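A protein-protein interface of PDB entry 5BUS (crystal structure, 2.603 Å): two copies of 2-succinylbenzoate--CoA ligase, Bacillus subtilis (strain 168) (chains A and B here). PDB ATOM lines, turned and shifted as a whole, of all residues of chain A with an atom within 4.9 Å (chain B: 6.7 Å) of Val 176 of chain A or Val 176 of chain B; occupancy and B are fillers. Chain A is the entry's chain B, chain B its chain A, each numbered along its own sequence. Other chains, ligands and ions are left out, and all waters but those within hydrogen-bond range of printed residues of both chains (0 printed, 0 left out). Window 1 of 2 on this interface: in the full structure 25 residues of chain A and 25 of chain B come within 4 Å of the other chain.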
ATOM      1  N   TYR A 172      19.059  21.788  18.754  1.00  0.00           N
ATOM      2  CA  TYR A 172      17.891  21.013  18.368  1.00  0.00           C
ATOM      3  C   TYR A 172      17.040  21.747  17.328  1.00  0.00           C
ATOM      4  O   TYR A 172      16.689  21.158  16.300  1.00  0.00           O
ATOM      5  CB  TYR A 172      17.038  20.673  19.586  1.00  0.00           C
ATOM      6  CG  TYR A 172      15.693  20.051  19.241  1.00  0.00           C
ATOM      7  CD1 TYR A 172      14.567  20.865  19.045  1.00  0.00           C
ATOM      8  CD2 TYR A 172      15.529  18.654  19.145  1.00  0.00           C
ATOM      9  CE1 TYR A 172      13.342  20.336  18.736  1.00  0.00           C
ATOM     10  CE2 TYR A 172      14.265  18.097  18.835  1.00  0.00           C
ATOM     11  CZ  TYR A 172      13.179  18.964  18.637  1.00  0.00           C
ATOM     12  OH  TYR A 172      11.922  18.516  18.323  1.00  0.00           O
ATOM     13  N   PHE A 173      16.693  23.016  17.587  1.00  0.00           N
ATOM     14  CA  PHE A 173      15.784  23.682  16.648  1.00  0.00           C
ATOM     15  C   PHE A 173      16.478  23.912  15.321  1.00  0.00           C
ATOM     16  O   PHE A 173      15.860  23.760  14.263  1.00  0.00           O
ATOM     17  CB  PHE A 173      15.199  24.983  17.239  1.00  0.00           C
ATOM     18  CG  PHE A 173      13.988  24.733  18.090  1.00  0.00           C
ATOM     19  CD1 PHE A 173      12.801  24.310  17.501  1.00  0.00           C
ATOM     20  CD2 PHE A 173      14.043  24.862  19.465  1.00  0.00           C
ATOM     21  CE1 PHE A 173      11.674  24.021  18.270  1.00  0.00           C
ATOM     22  CE2 PHE A 173      12.919  24.581  20.256  1.00  0.00           C
ATOM     23  CZ  PHE A 173      11.730  24.148  19.648  1.00  0.00           C
ATOM     24  N   SER A 174      17.773  24.212  15.370  1.00  0.00           N
ATOM     25  CA  SER A 174      18.560  24.296  14.150  1.00  0.00           C
ATOM     26  C   SER A 174      18.490  23.004  13.328  1.00  0.00           C
ATOM     27  O   SER A 174      18.307  23.041  12.114  1.00  0.00           O
ATOM     28  CB  SER A 174      20.020  24.613  14.475  1.00  0.00           C
ATOM     29  OG  SER A 174      20.789  24.652  13.288  1.00  0.00           O
ATOM     30  N   ALA A 175      18.637  21.858  13.989  1.00  0.00           N
ATOM     31  CA  ALA A 175      18.641  20.568  13.288  1.00  0.00           C
ATOM     32  C   ALA A 175      17.248  20.211  12.747  1.00  0.00           C
ATOM     33  O   ALA A 175      17.111  19.694  11.637  1.00  0.00           O
ATOM     34  CB  ALA A 175      19.159  19.468  14.216  1.00  0.00           C
ATOM     35  N   VAL A 176      16.216  20.506  13.531  1.00  0.00           N
ATOM     36  CA  VAL A 176      14.835  20.260  13.120  1.00  0.00           C
ATOM     37  C   VAL A 176      14.405  21.175  11.961  1.00  0.00           C
ATOM     38  O   VAL A 176      13.791  20.711  10.994  1.00  0.00           O
ATOM     39  CB  VAL A 176      13.877  20.439  14.307  1.00  0.00           C
ATOM     40  CG1 VAL A 176      12.458  20.584  13.831  1.00  0.00           C
ATOM     41  CG2 VAL A 176      14.047  19.282  15.307  1.00  0.00           C
ATOM     42  N   SER A 177      14.737  22.460  12.046  1.00  0.00           N
ATOM     43  CA  SER A 177      14.420  23.408  10.975  1.00  0.00           C
ATOM     44  C   SER A 177      15.078  23.034   9.646  1.00  0.00           C
ATOM     45  O   SER A 177      14.457  23.130   8.585  1.00  0.00           O
ATOM     46  CB  SER A 177      14.839  24.822  11.373  1.00  0.00           C
ATOM     47  OG  SER A 177      13.955  25.331  12.356  1.00  0.00           O
ATOM     48  N   SER A 178      16.336  22.611   9.709  1.00  0.00           N
ATOM     49  CA  SER A 178      17.074  22.192   8.515  1.00  0.00           C
ATOM     50  C   SER A 178      16.456  20.956   7.866  1.00  0.00           C
ATOM     51  O   SER A 178      16.415  20.854   6.639  1.00  0.00           O
ATOM     52  CB  SER A 178      18.546  21.923   8.864  1.00  0.00           C
ATOM     53  OG  SER A 178      19.292  21.570   7.715  1.00  0.00           O
ATOM     54  N   ALA A 179      15.980  20.021   8.691  1.00  0.00           N
ATOM     55  CA  ALA A 179      15.309  18.815   8.189  1.00  0.00           C
ATOM     56  C   ALA A 179      14.018  19.167   7.460  1.00  0.00           C
ATOM     57  O   ALA A 179      13.747  18.631   6.388  1.00  0.00           O
ATOM     58  CB  ALA A 179      15.021  17.821   9.336  1.00  0.00           C
ATOM     59  N   LEU A 180      13.222  20.058   8.048  1.00  0.00           N
ATOM     60  CA  LEU A 180      12.000  20.558   7.414  1.00  0.00           C
ATOM     61  C   LEU A 180      12.343  21.200   6.073  1.00  0.00           C
ATOM     62  O   LEU A 180      11.570  21.150   5.123  1.00  0.00           O
ATOM     63  CB  LEU A 180      11.288  21.562   8.325  1.00  0.00           C
ATOM     64  CG  LEU A 180      10.827  21.015   9.689  1.00  0.00           C
ATOM     65  CD1 LEU A 180      10.182  22.105  10.546  1.00  0.00           C
ATOM     66  CD2 LEU A 180       9.871  19.831   9.547  1.00  0.00           C
ATOM     67  N   TYR A 211      18.819  13.000  14.154  1.00  0.00           N
ATOM     68  CA  TYR A 211      18.259  12.235  13.035  1.00  0.00           C
ATOM     69  C   TYR A 211      18.612  10.736  13.140  1.00  0.00           C
ATOM     70  O   TYR A 211      17.890   9.897  12.648  1.00  0.00           O
ATOM     71  CB  TYR A 211      18.750  12.727  11.682  1.00  0.00           C
ATOM     72  CG  TYR A 211      18.657  14.206  11.362  1.00  0.00           C
ATOM     73  CD1 TYR A 211      17.935  15.105  12.146  1.00  0.00           C
ATOM     74  CD2 TYR A 211      19.350  14.710  10.264  1.00  0.00           C
ATOM     75  CE1 TYR A 211      17.896  16.477  11.807  1.00  0.00           C
ATOM     76  CE2 TYR A 211      19.323  16.048   9.932  1.00  0.00           C
ATOM     77  CZ  TYR A 211      18.602  16.923  10.686  1.00  0.00           C
ATOM     78  OH  TYR A 211      18.611  18.233  10.286  1.00  0.00           O
ATOM     79  N   HIS B 171       1.453  20.030  19.380  1.00  0.00           N
ATOM     80  CA  HIS B 171       1.256  19.681  17.980  1.00  0.00           C
ATOM     81  C   HIS B 171       2.549  19.783  17.179  1.00  0.00           C
ATOM     82  O   HIS B 171       2.868  18.892  16.385  1.00  0.00           O
ATOM     83  CB  HIS B 171       0.178  20.570  17.350  1.00  0.00           C
ATOM     84  CG  HIS B 171      -1.198  20.338  17.907  1.00  0.00           C
ATOM     85  ND1 HIS B 171      -1.728  19.077  18.080  1.00  0.00           N
ATOM     86  CD2 HIS B 171      -2.149  21.204  18.326  1.00  0.00           C
ATOM     87  CE1 HIS B 171      -2.947  19.177  18.583  1.00  0.00           C
ATOM     88  NE2 HIS B 171      -3.227  20.456  18.744  1.00  0.00           N
ATOM     89  N   TYR B 172       3.304  20.853  17.395  1.00  0.00           N
ATOM     90  CA  TYR B 172       4.575  21.012  16.681  1.00  0.00           C
ATOM     91  C   TYR B 172       5.511  19.836  16.992  1.00  0.00           C
ATOM     92  O   TYR B 172       6.124  19.239  16.100  1.00  0.00           O
ATOM     93  CB  TYR B 172       5.253  22.338  17.042  1.00  0.00           C
ATOM     94  CG  TYR B 172       6.705  22.420  16.607  1.00  0.00           C
ATOM     95  CD1 TYR B 172       7.052  22.908  15.343  1.00  0.00           C
ATOM     96  CD2 TYR B 172       7.728  22.012  17.459  1.00  0.00           C
ATOM     97  CE1 TYR B 172       8.379  22.977  14.939  1.00  0.00           C
ATOM     98  CE2 TYR B 172       9.056  22.071  17.068  1.00  0.00           C
ATOM     99  CZ  TYR B 172       9.377  22.565  15.816  1.00  0.00           C
ATOM    100  OH  TYR B 172      10.702  22.630  15.432  1.00  0.00           O
ATOM    101  N   PHE B 173       5.619  19.515  18.268  1.00  0.00           N
ATOM    102  CA  PHE B 173       6.558  18.486  18.680  1.00  0.00           C
ATOM    103  C   PHE B 173       6.127  17.088  18.231  1.00  0.00           C
ATOM    104  O   PHE B 173       6.965  16.281  17.792  1.00  0.00           O
ATOM    105  CB  PHE B 173       6.791  18.572  20.197  1.00  0.00           C
ATOM    106  CG  PHE B 173       7.844  19.574  20.548  1.00  0.00           C
ATOM    107  CD1 PHE B 173       9.175  19.309  20.251  1.00  0.00           C
ATOM    108  CD2 PHE B 173       7.519  20.779  21.136  1.00  0.00           C
ATOM    109  CE1 PHE B 173      10.168  20.226  20.544  1.00  0.00           C
ATOM    110  CE2 PHE B 173       8.510  21.713  21.438  1.00  0.00           C
ATOM    111  CZ  PHE B 173       9.840  21.439  21.135  1.00  0.00           C
ATOM    112  N   SER B 174       4.826  16.828  18.291  1.00  0.00           N
ATOM    113  CA  SER B 174       4.234  15.653  17.648  1.00  0.00           C
ATOM    114  C   SER B 174       4.674  15.519  16.205  1.00  0.00           C
ATOM    115  O   SER B 174       5.247  14.492  15.839  1.00  0.00           O
ATOM    116  CB  SER B 174       2.717  15.722  17.707  1.00  0.00           C
ATOM    117  OG  SER B 174       2.187  14.459  17.390  1.00  0.00           O
ATOM    118  N   ALA B 175       4.464  16.570  15.404  1.00  0.00           N
ATOM    119  CA  ALA B 175       4.819  16.547  13.982  1.00  0.00           C
ATOM    120  C   ALA B 175       6.315  16.294  13.783  1.00  0.00           C
ATOM    121  O   ALA B 175       6.719  15.440  12.981  1.00  0.00           O
ATOM    122  CB  ALA B 175       4.397  17.868  13.294  1.00  0.00           C
ATOM    123  N   VAL B 176       7.138  17.019  14.534  1.00  0.00           N
ATOM    124  CA  VAL B 176       8.585  16.950  14.375  1.00  0.00           C
ATOM    125  C   VAL B 176       9.102  15.586  14.803  1.00  0.00           C
ATOM    126  O   VAL B 176       9.877  14.928  14.107  1.00  0.00           O
ATOM    127  CB  VAL B 176       9.286  18.036  15.207  1.00  0.00           C
ATOM    128  CG1 VAL B 176      10.781  17.741  15.322  1.00  0.00           C
ATOM    129  CG2 VAL B 176       9.022  19.405  14.604  1.00  0.00           C
ATOM    130  N   SER B 177       8.638  15.153  15.958  1.00  0.00           N
ATOM    131  CA  SER B 177       9.122  13.920  16.537  1.00  0.00           C
ATOM    132  C   SER B 177       8.747  12.740  15.608  1.00  0.00           C
ATOM    133  O   SER B 177       9.495  11.774  15.458  1.00  0.00           O
ATOM    134  CB  SER B 177       8.546  13.780  17.954  1.00  0.00           C
ATOM    135  OG  SER B 177       9.202  12.810  18.732  1.00  0.00           O
ATOM    136  N   SER B 178       7.610  12.859  14.937  1.00  0.00           N
ATOM    137  CA  SER B 178       7.152  11.824  14.021  1.00  0.00           C
ATOM    138  C   SER B 178       8.015  11.804  12.767  1.00  0.00           C
ATOM    139  O   SER B 178       8.347  10.729  12.237  1.00  0.00           O
ATOM    140  CB  SER B 178       5.680  12.060  13.657  1.00  0.00           C
ATOM    141  OG  SER B 178       5.163  11.015  12.875  1.00  0.00           O
ATOM    142  N   ALA B 179       8.384  12.989  12.289  1.00  0.00           N
ATOM    143  CA  ALA B 179       9.235  13.079  11.090  1.00  0.00           C
ATOM    144  C   ALA B 179      10.607  12.470  11.336  1.00  0.00           C
ATOM    145  O   ALA B 179      11.228  11.949  10.412  1.00  0.00           O
ATOM    146  CB  ALA B 179       9.382  14.534  10.636  1.00  0.00           C
ATOM    147  N   LEU B 180      11.091  12.545  12.576  1.00  0.00           N
ATOM    148  CA  LEU B 180      12.385  11.935  12.899  1.00  0.00           C
ATOM    149  C   LEU B 180      12.244  10.426  12.998  1.00  0.00           C
ATOM    150  O   LEU B 180      13.229   9.709  12.920  1.00  0.00           O
ATOM    151  CB  LEU B 180      12.958  12.490  14.210  1.00  0.00           C
ATOM    152  CG  LEU B 180      13.221  14.004  14.177  1.00  0.00           C
ATOM    153  CD1 LEU B 180      13.565  14.512  15.549  1.00  0.00           C
ATOM    154  CD2 LEU B 180      14.321  14.358  13.199  1.00  0.00           C
ATOM    155  N   ASN B 181      11.023   9.949  13.218  1.00  0.00           N
ATOM    156  CA  ASN B 181      10.762   8.518  13.273  1.00  0.00           C
ATOM    157  C   ASN B 181      10.609   7.991  11.839  1.00  0.00           C
ATOM    158  O   ASN B 181      11.137   6.945  11.513  1.00  0.00           O
ATOM    159  CB  ASN B 181       9.494   8.234  14.114  1.00  0.00           C
ATOM    160  CG  ASN B 181       9.190   6.738  14.278  1.00  0.00           C
ATOM    161  OD1 ASN B 181       8.064   6.301  14.104  1.00  0.00           O
ATOM    162  ND2 ASN B 181      10.198   5.963  14.626  1.00  0.00           N
ATOM    163  N   ILE B 184      11.022  12.489   6.180  1.00  0.00           N
ATOM    164  CA  ILE B 184      10.119  13.287   5.347  1.00  0.00           C
ATOM    165  C   ILE B 184      10.785  13.654   4.014  1.00  0.00           C
ATOM    166  O   ILE B 184      11.940  14.099   3.996  1.00  0.00           O
ATOM    167  CB  ILE B 184       9.681  14.571   6.067  1.00  0.00           C
ATOM    168  CG1 ILE B 184      10.874  15.230   6.760  1.00  0.00           C
ATOM    169  CG2 ILE B 184       8.672  14.250   7.125  1.00  0.00           C
ATOM    170  CD1 ILE B 184      10.507  16.439   7.588  1.00  0.00           C
ATOM    171  N   LYS B 207       0.937  18.404  10.554  1.00  0.00           N
ATOM    172  CA  LYS B 207       2.061  17.826   9.806  1.00  0.00           C
ATOM    173  C   LYS B 207       2.166  18.509   8.451  1.00  0.00           C
ATOM    174  O   LYS B 207       3.251  18.892   8.024  1.00  0.00           O
ATOM    175  CB  LYS B 207       1.908  16.314   9.602  1.00  0.00           C
ATOM    176  CG  LYS B 207       2.238  15.438  10.818  1.00  0.00           C
ATOM    177  CD  LYS B 207       2.046  13.932  10.497  1.00  0.00           C
ATOM    178  CE  LYS B 207       2.139  13.066  11.760  1.00  0.00           C
ATOM    179  NZ  LYS B 207       0.784  12.657  12.282  1.00  0.00           N
ATOM    180  N   ILE B 210       3.476  22.271   8.547  1.00  0.00           N
ATOM    181  CA  ILE B 210       4.839  22.291   9.079  1.00  0.00           C
ATOM    182  C   ILE B 210       5.814  21.638   8.109  1.00  0.00           C
ATOM    183  O   ILE B 210       6.899  22.190   7.860  1.00  0.00           O
ATOM    184  CB  ILE B 210       4.933  21.594  10.455  1.00  0.00           C
ATOM    185  CG1 ILE B 210       4.199  22.426  11.525  1.00  0.00           C
ATOM    186  CG2 ILE B 210       6.402  21.408  10.843  1.00  0.00           C
ATOM    187  CD1 ILE B 210       3.811  21.658  12.780  1.00  0.00           C
ATOM    188  N   TYR B 211       5.435  20.481   7.550  1.00  0.00           N
ATOM    189  CA  TYR B 211       6.300  19.830   6.562  1.00  0.00           C
ATOM    190  C   TYR B 211       6.193  20.481   5.180  1.00  0.00           C
ATOM    191  O   TYR B 211       7.117  20.376   4.371  1.00  0.00           O
ATOM    192  CB  TYR B 211       5.991  18.340   6.374  1.00  0.00           C
ATOM    193  CG  TYR B 211       5.975  17.432   7.577  1.00  0.00           C
ATOM    194  CD1 TYR B 211       6.478  17.827   8.804  1.00  0.00           C
ATOM    195  CD2 TYR B 211       5.464  16.134   7.454  1.00  0.00           C
ATOM    196  CE1 TYR B 211       6.447  16.956   9.895  1.00  0.00           C
ATOM    197  CE2 TYR B 211       5.436  15.272   8.505  1.00  0.00           C
ATOM    198  CZ  TYR B 211       5.926  15.671   9.730  1.00  0.00           C
ATOM    199  OH  TYR B 211       5.873  14.760  10.763  1.00  0.00           O
ATOM    200  N   PHE B 317      11.476  10.051  19.171  1.00  0.00           N
ATOM    201  CA  PHE B 317      12.580  10.848  19.670  1.00  0.00           C
ATOM    202  C   PHE B 317      12.012  11.998  20.507  1.00  0.00           C
ATOM    203  O   PHE B 317      10.909  12.461  20.238  1.00  0.00           O
ATOM    204  CB  PHE B 317      13.437  11.361  18.527  1.00  0.00           C
ATOM    205  CG  PHE B 317      14.836  11.660  18.926  1.00  0.00           C
ATOM    206  CD1 PHE B 317      15.776  10.644  18.968  1.00  0.00           C
ATOM    207  CD2 PHE B 317      15.215  12.954  19.275  1.00  0.00           C
ATOM    208  CE1 PHE B 317      17.077  10.902  19.353  1.00  0.00           C
ATOM    209  CE2 PHE B 317      16.515  13.224  19.651  1.00  0.00           C
ATOM    210  CZ  PHE B 317      17.456  12.195  19.691  1.00  0.00           C
ATOM    211  N   SER B 318      12.751  12.397  21.550  1.00  0.00           N
ATOM    212  CA  SER B 318      12.309  13.399  22.538  1.00  0.00           C
ATOM    213  C   SER B 318      11.271  12.879  23.550  1.00  0.00           C
ATOM    214  O   SER B 318      10.836  13.632  24.412  1.00  0.00           O
ATOM    215  CB  SER B 318      11.720  14.638  21.850  1.00  0.00           C
ATOM    216  OG  SER B 318      12.499  15.031  20.750  1.00  0.00           O
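Of the 17 printed residues of chain B, 6 touch a printed residue of chain A. Printed residues of chain B that touch a printed residue of chain A: Tyr 172, Phe 173, Val 176, Leu 180, Ile 184 and Ile 210. Hydrophobic or aromatic side chains of chain B within 4 Å of the printed part of chain A: Tyr 172, Phe 173, Val 176, Leu 180, Ile 184 and Ile 210. Among the printed residues, no Asp or Glu carboxylate lies within 4 Å of a Lys or Arg side-chain nitrogen of the other chain.
Of chain B, only Tyr 172 (3.1 Å) and Val 176 (3.6 Å) come within 4 Å of Val 176 of chain A. Of the printed residues of chain B, Leu 180 of chain A touches Ile 184 and Ile 210. Of the printed residues of chain B, Tyr 211 of chain A touches Leu 180. Ala 175 of chain B touches none of the printed residues of chain A. Printed residues of chain A within 4 Å of Val 176 of chain B: Tyr 172 (3.3 Å) and Val 176 (3.6 Å). Of the printed residues of chain A, Ile 210 of chain B touches Leu 180. The nearest printed residue of chain A that does not touch Val 176 of chain B is Leu 180 of chain A (5.0 Å). The nearest printed residue of chain A that does not touch Tyr 172 of chain B is Tyr 172 of chain A (4.7 Å).
Tyr 172 of chain A touches Phe 173 of chain B, and with the chains exchanged Phe 173 of chain A touches Tyr 172 of chain B. Tyr 172 of chain A touches Val 176 of chain B, and with the chains exchanged Val 176 of chain A touches Tyr 172 of chain B. Phe 173 of chain B touches its own counterpart, Phe 173 of chain A. Val 176 of chain A touches its own counterpart, Val 176 of chain B. 10 positions are printed for both chains. Of the 9 pairs that touch across the chains among the printed residues, 6 have their exchanged pair printed and touching as well.
O of Phe 173 of chain A sits at hydrogen-bond distance from OG of Ser 177 of chain A, at 3.1 Å. The backbone carbonyl oxygen (O) of Ala 175 of chain A lies within hydrogen-bond range of the side-chain hydroxyl (OH) of Tyr 211 of chain A.
Among the printed residues, merely in contact across the chains: Tyr 172 of chain A with Phe 173 of chain B, Tyr 172 of chain A with Val 176 of chain B, Phe 173 of chain A with Tyr 172 of chain B, Phe 173 of chain A with Phe 173 of chain B, Val 176 of chain A with Tyr 172 of chain B, Val 176 of chain A with Val 176 of chain B, Leu 180 of chain A with Ile 184 of chain B, Leu 180 of chain A with Ile 210 of chain B and Tyr 211 of chain A with Leu 180 of chain B.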
